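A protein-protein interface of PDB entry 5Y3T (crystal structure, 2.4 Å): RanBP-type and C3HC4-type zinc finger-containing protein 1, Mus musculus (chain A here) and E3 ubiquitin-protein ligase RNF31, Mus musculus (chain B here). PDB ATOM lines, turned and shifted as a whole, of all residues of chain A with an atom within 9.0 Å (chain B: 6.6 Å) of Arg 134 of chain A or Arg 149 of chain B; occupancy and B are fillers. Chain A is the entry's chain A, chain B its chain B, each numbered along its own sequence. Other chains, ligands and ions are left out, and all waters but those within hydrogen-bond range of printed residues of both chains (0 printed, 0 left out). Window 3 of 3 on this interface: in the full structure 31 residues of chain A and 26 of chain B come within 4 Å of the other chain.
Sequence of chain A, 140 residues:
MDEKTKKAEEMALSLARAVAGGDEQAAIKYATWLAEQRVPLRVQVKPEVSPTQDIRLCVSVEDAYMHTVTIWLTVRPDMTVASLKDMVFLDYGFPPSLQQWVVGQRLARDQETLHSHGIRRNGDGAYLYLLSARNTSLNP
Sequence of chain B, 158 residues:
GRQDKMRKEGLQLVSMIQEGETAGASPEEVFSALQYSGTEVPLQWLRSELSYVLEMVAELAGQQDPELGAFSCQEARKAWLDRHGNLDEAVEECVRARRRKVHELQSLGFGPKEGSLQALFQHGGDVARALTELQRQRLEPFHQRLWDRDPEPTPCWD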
ATOM      1  N   ALA A  64       3.983  11.873  11.417  1.00  0.00           N
ATOM      2  CA  ALA A  64       3.199  12.056  10.207  1.00  0.00           C
ATOM      3  C   ALA A  64       3.782  13.034   9.219  1.00  0.00           C
ATOM      4  O   ALA A  64       3.076  13.483   8.317  1.00  0.00           O
ATOM      5  CB  ALA A  64       1.784  12.499  10.612  1.00  0.00           C
ATOM      6  N   TYR A  65       5.049  13.414   9.387  1.00  0.00           N
ATOM      7  CA  TYR A  65       5.697  14.420   8.532  1.00  0.00           C
ATOM      8  C   TYR A  65       7.044  13.898   8.040  1.00  0.00           C
ATOM      9  O   TYR A  65       7.919  14.693   7.630  1.00  0.00           O
ATOM     10  CB  TYR A  65       5.818  15.751   9.304  1.00  0.00           C
ATOM     11  CG  TYR A  65       4.463  16.269   9.781  1.00  0.00           C
ATOM     12  CD1 TYR A  65       3.905  15.864  10.999  1.00  0.00           C
ATOM     13  CD2 TYR A  65       3.724  17.136   8.990  1.00  0.00           C
ATOM     14  CE1 TYR A  65       2.630  16.314  11.395  1.00  0.00           C
ATOM     15  CE2 TYR A  65       2.481  17.591   9.388  1.00  0.00           C
ATOM     16  CZ  TYR A  65       1.927  17.187  10.581  1.00  0.00           C
ATOM     17  OH  TYR A  65       0.654  17.696  10.920  1.00  0.00           O
ATOM     18  N   LEU A  98      -2.920   9.803  19.887  1.00  0.00           N
ATOM     19  CA  LEU A  98      -2.040   9.949  18.711  1.00  0.00           C
ATOM     20  C   LEU A  98      -0.818   9.021  18.677  1.00  0.00           C
ATOM     21  O   LEU A  98       0.015   9.103  17.745  1.00  0.00           O
ATOM     22  CB  LEU A  98      -1.605  11.396  18.566  1.00  0.00           C
ATOM     23  CG  LEU A  98      -2.683  12.467  18.573  1.00  0.00           C
ATOM     24  CD1 LEU A  98      -2.012  13.822  18.419  1.00  0.00           C
ATOM     25  CD2 LEU A  98      -3.695  12.221  17.460  1.00  0.00           C
ATOM     26  N   LEU A 131       0.820  10.382  15.335  1.00  0.00           N
ATOM     27  CA  LEU A 131      -0.147  10.892  14.391  1.00  0.00           C
ATOM     28  C   LEU A 131      -0.252  12.395  14.538  1.00  0.00           C
ATOM     29  O   LEU A 131      -0.167  12.923  15.640  1.00  0.00           O
ATOM     30  CB  LEU A 131      -1.527  10.257  14.673  1.00  0.00           C
ATOM     31  CG  LEU A 131      -1.599   8.769  14.360  1.00  0.00           C
ATOM     32  CD1 LEU A 131      -2.635   8.089  15.222  1.00  0.00           C
ATOM     33  CD2 LEU A 131      -1.900   8.545  12.881  1.00  0.00           C
ATOM     34  N   SER A 132      -0.472  13.076  13.418  1.00  0.00           N
ATOM     35  CA  SER A 132      -0.864  14.457  13.417  1.00  0.00           C
ATOM     36  C   SER A 132      -2.248  14.613  14.027  1.00  0.00           C
ATOM     37  O   SER A 132      -3.093  13.716  13.910  1.00  0.00           O
ATOM     38  CB  SER A 132      -0.886  15.009  11.995  1.00  0.00           C
ATOM     39  OG  SER A 132      -1.463  16.307  11.937  1.00  0.00           O
ATOM     40  N   ALA A 133      -2.440  15.761  14.681  1.00  0.00           N
ATOM     41  CA  ALA A 133      -3.740  16.264  15.123  1.00  0.00           C
ATOM     42  C   ALA A 133      -4.672  16.546  13.953  1.00  0.00           C
ATOM     43  O   ALA A 133      -5.837  16.752  14.160  1.00  0.00           O
ATOM     44  CB  ALA A 133      -3.568  17.556  15.935  1.00  0.00           C
ATOM     45  N   ARG A 134      -4.155  16.659  12.746  1.00  0.00           N
ATOM     46  CA  ARG A 134      -5.006  16.820  11.575  1.00  0.00           C
ATOM     47  C   ARG A 134      -5.432  15.491  10.921  1.00  0.00           C
ATOM     48  O   ARG A 134      -6.379  15.501  10.145  1.00  0.00           O
ATOM     49  CB  ARG A 134      -4.295  17.671  10.553  1.00  0.00           C
ATOM     50  CG  ARG A 134      -3.992  19.064  11.049  1.00  0.00           C
ATOM     51  CD  ARG A 134      -3.348  19.823   9.908  1.00  0.00           C
ATOM     52  NE  ARG A 134      -3.178  21.231  10.220  1.00  0.00           N
ATOM     53  CZ  ARG A 134      -4.108  22.173  10.074  1.00  0.00           C
ATOM     54  NH1 ARG A 134      -5.333  21.896   9.632  1.00  0.00           N
ATOM     55  NH2 ARG A 134      -3.804  23.418  10.397  1.00  0.00           N
ATOM     56  N   ASN A 135      -4.762  14.369  11.229  1.00  0.00           N
ATOM     57  CA  ASN A 135      -5.212  13.021  10.757  1.00  0.00           C
ATOM     58  C   ASN A 135      -6.634  12.734  11.228  1.00  0.00           C
ATOM     59  O   ASN A 135      -6.935  12.853  12.413  1.00  0.00           O
ATOM     60  CB  ASN A 135      -4.276  11.879  11.195  1.00  0.00           C
ATOM     61  CG  ASN A 135      -2.982  11.787  10.341  1.00  0.00           C
ATOM     62  OD1 ASN A 135      -2.969  12.099   9.144  1.00  0.00           O
ATOM     63  ND2 ASN A 135      -1.899  11.334  10.962  1.00  0.00           N
ATOM     64  N   THR A 136      -7.469  12.312  10.279  1.00  0.00           N
ATOM     65  CA  THR A 136      -8.926  12.517  10.318  1.00  0.00           C
ATOM     66  C   THR A 136      -9.690  11.524  11.201  1.00  0.00           C
ATOM     67  O   THR A 136      -9.405  10.331  11.198  1.00  0.00           O
ATOM     68  CB  THR A 136      -9.479  12.486   8.870  1.00  0.00           C
ATOM     69  OG1 THR A 136      -8.802  11.461   8.122  1.00  0.00           O
ATOM     70  CG2 THR A 136      -9.240  13.835   8.164  1.00  0.00           C
ATOM     71  N   ARG B 145       5.488  19.985  15.699  1.00  0.00           N
ATOM     72  CA  ARG B 145       4.945  19.711  14.337  1.00  0.00           C
ATOM     73  C   ARG B 145       3.480  19.176  14.281  1.00  0.00           C
ATOM     74  O   ARG B 145       2.881  19.101  13.236  1.00  0.00           O
ATOM     75  CB  ARG B 145       5.837  18.670  13.604  1.00  0.00           C
ATOM     76  CG  ARG B 145       7.049  19.226  12.904  1.00  0.00           C
ATOM     77  CD  ARG B 145       7.734  18.137  12.105  1.00  0.00           C
ATOM     78  NE  ARG B 145       8.286  17.044  12.907  1.00  0.00           N
ATOM     79  CZ  ARG B 145       9.522  17.008  13.443  1.00  0.00           C
ATOM     80  NH1 ARG B 145      10.371  18.021  13.334  1.00  0.00           N
ATOM     81  NH2 ARG B 145       9.909  15.944  14.130  1.00  0.00           N
ATOM     82  N   LEU B 146       2.906  18.801  15.401  1.00  0.00           N
ATOM     83  CA  LEU B 146       1.688  18.009  15.389  1.00  0.00           C
ATOM     84  C   LEU B 146       0.513  18.587  14.611  1.00  0.00           C
ATOM     85  O   LEU B 146      -0.352  17.840  14.212  1.00  0.00           O
ATOM     86  CB  LEU B 146       1.247  17.727  16.831  1.00  0.00           C
ATOM     87  CG  LEU B 146       2.144  16.773  17.582  1.00  0.00           C
ATOM     88  CD1 LEU B 146       1.646  16.714  19.000  1.00  0.00           C
ATOM     89  CD2 LEU B 146       2.187  15.374  16.950  1.00  0.00           C
ATOM     90  N   TRP B 147       0.464  19.898  14.454  1.00  0.00           N
ATOM     91  CA  TRP B 147      -0.677  20.589  13.870  1.00  0.00           C
ATOM     92  C   TRP B 147      -0.274  21.209  12.548  1.00  0.00           C
ATOM     93  O   TRP B 147      -0.949  22.110  12.095  1.00  0.00           O
ATOM     94  CB  TRP B 147      -1.147  21.709  14.822  1.00  0.00           C
ATOM     95  CG  TRP B 147      -1.762  21.205  16.093  1.00  0.00           C
ATOM     96  CD1 TRP B 147      -1.114  20.619  17.163  1.00  0.00           C
ATOM     97  CD2 TRP B 147      -3.178  21.194  16.432  1.00  0.00           C
ATOM     98  NE1 TRP B 147      -2.047  20.227  18.137  1.00  0.00           N
ATOM     99  CE2 TRP B 147      -3.306  20.585  17.715  1.00  0.00           C
ATOM    100  CE3 TRP B 147      -4.331  21.646  15.781  1.00  0.00           C
ATOM    101  CZ2 TRP B 147      -4.529  20.428  18.350  1.00  0.00           C
ATOM    102  CZ3 TRP B 147      -5.547  21.492  16.420  1.00  0.00           C
ATOM    103  CH2 TRP B 147      -5.641  20.877  17.690  1.00  0.00           C
ATOM    104  N   ASP B 148       0.837  20.773  11.948  1.00  0.00           N
ATOM    105  CA  ASP B 148       1.305  21.345  10.662  1.00  0.00           C
ATOM    106  C   ASP B 148       0.375  20.911   9.511  1.00  0.00           C
ATOM    107  O   ASP B 148      -0.174  19.784   9.538  1.00  0.00           O
ATOM    108  CB  ASP B 148       2.742  20.882  10.313  1.00  0.00           C
ATOM    109  CG  ASP B 148       3.837  21.658  11.040  1.00  0.00           C
ATOM    110  OD1 ASP B 148       3.551  22.532  11.886  1.00  0.00           O
ATOM    111  OD2 ASP B 148       5.020  21.355  10.783  1.00  0.00           O
ATOM    112  N   ARG B 149       0.242  21.799   8.512  1.00  0.00           N
ATOM    113  CA  ARG B 149      -0.507  21.541   7.261  1.00  0.00           C
ATOM    114  C   ARG B 149      -0.019  20.278   6.611  1.00  0.00           C
ATOM    115  O   ARG B 149       1.180  20.027   6.590  1.00  0.00           O
ATOM    116  CB  ARG B 149      -0.287  22.666   6.235  1.00  0.00           C
ATOM    117  CG  ARG B 149      -1.034  23.957   6.517  1.00  0.00           C
ATOM    118  CD  ARG B 149      -0.532  25.110   5.649  1.00  0.00           C
ATOM    119  NE  ARG B 149      -1.075  26.396   6.103  1.00  0.00           N
ATOM    120  CZ  ARG B 149      -0.745  27.601   5.624  1.00  0.00           C
ATOM    121  NH1 ARG B 149       0.143  27.737   4.643  1.00  0.00           N
ATOM    122  NH2 ARG B 149      -1.318  28.693   6.129  1.00  0.00           N
ATOM    123  N   ASP B 150      -0.948  19.475   6.106  1.00  0.00           N
ATOM    124  CA  ASP B 150      -0.648  18.415   5.137  1.00  0.00           C
ATOM    125  C   ASP B 150       0.148  17.235   5.695  1.00  0.00           C
ATOM    126  O   ASP B 150       1.167  16.852   5.134  1.00  0.00           O
ATOM    127  CB  ASP B 150       0.024  19.013   3.854  1.00  0.00           C
ATOM    128  CG  ASP B 150      -1.001  19.620   2.856  1.00  0.00           C
ATOM    129  OD1 ASP B 150      -1.950  20.348   3.260  1.00  0.00           O
ATOM    130  OD2 ASP B 150      -0.852  19.352   1.643  1.00  0.00           O
ATOM    131  N   PRO B 151      -0.319  16.634   6.797  1.00  0.00           N
ATOM    132  CA  PRO B 151       0.408  15.473   7.247  1.00  0.00           C
ATOM    133  C   PRO B 151       0.227  14.329   6.259  1.00  0.00           C
ATOM    134  O   PRO B 151      -0.718  14.351   5.439  1.00  0.00           O
ATOM    135  CB  PRO B 151      -0.301  15.108   8.558  1.00  0.00           C
ATOM    136  CG  PRO B 151      -1.702  15.574   8.382  1.00  0.00           C
ATOM    137  CD  PRO B 151      -1.554  16.848   7.585  1.00  0.00           C
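O of Leu 146 of chain B is in hydrogen-bond range of N of Ala 133 of chain A.
O of Trp 147 of chain B sits at hydrogen-bond distance from NE of Arg 134 of chain A (3.0 Å).
O of Leu 146 of chain B is in hydrogen-bond range of OH of Tyr 65 of chain A (3.4 Å).
The guanidinium group of Arg 134 of chain A sits close to the backbone carbonyl oxygen of Asp 148 of chain B (3.4 Å).
The side-chain hydroxyl (OG) of Ser 132 of chain A is in hydrogen-bond range of the backbone carbonyl oxygen (O) of Leu 146 of chain B.
The side-chain hydroxyl of Tyr 65 of chain A is in hydrogen-bond range of the backbone carbonyl oxygen of Asp 148 of chain B (2.6 Å).
The side-chain hydroxyl (OG) of Ser 132 of chain A sits at hydrogen-bond distance from the backbone NH (N) of Arg 134 of chain A, at 2.8 Å.
The side-chain hydroxyl (OG) of Ser 132 of chain A lies within hydrogen-bond range of the side-chain hydroxyl (OH) of Tyr 65 of chain A (2.7 Å).
N of Ser 132 of chain A sits close to ND2 of Asn 135 of chain A (3.3 Å).
O of Leu 98 of chain A sits at hydrogen-bond distance from N of Leu 131 of chain A (2.8 Å).
Among the printed residues, merely in contact across the chains: Ala 64 of chain A with Pro 151 of chain B (3.5 Å), Tyr 65 of chain A with Arg 145 of chain B (3.3 Å), Tyr 65 of chain A with Trp 147 of chain B (3.98 Å), Tyr 65 of chain A with Arg 149 of chain B (3.9 Å), Tyr 65 of chain A with Pro 151 of chain B (3.6 Å), Leu 131 of chain A with Leu 146 of chain B (3.6 Å), Ser 132 of chain A with Pro 151 of chain B (3.5 Å), Ala 133 of chain A with Trp 147 of chain B (3.5 Å), Arg 134 of chain A with Arg 149 of chain B (3.9 Å), Arg 134 of chain A with Pro 151 of chain B (3.98 Å) and Asn 135 of chain A with Pro 151 of chain B (3.8 Å).
Of the printed residues of chain B, Ala 64 of chain A touches Pro 151.
Of the printed residues of chain B, Leu 131 of chain A touches Leu 146 (3.6 Å).
Of the printed residues of chain B, Asn 135 of chain A touches Pro 151.
Of the printed residues of chain A, Arg 145 of chain B touches Tyr 65.
Arg 149 of chain B touches two residues of chain A.
The nearest residue of chain B that does not touch Arg 134 of chain A is Leu 146 of chain B (4.2 Å).
The nearest residue of chain A that does not touch Arg 149 of chain B is Ser 132 of chain A (6.7 Å).
Hydrophobic or aromatic side chains of chain A that line the printed part of chain B: Ala 64, Tyr 65 and Ala 133.
Of the 7 printed residues of chain B, 6 touch a printed residue of chain A.
Among the printed residues, no Asp or Glu carboxylate lies within 4 Å of a Lys or Arg side-chain nitrogen of the other chain.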
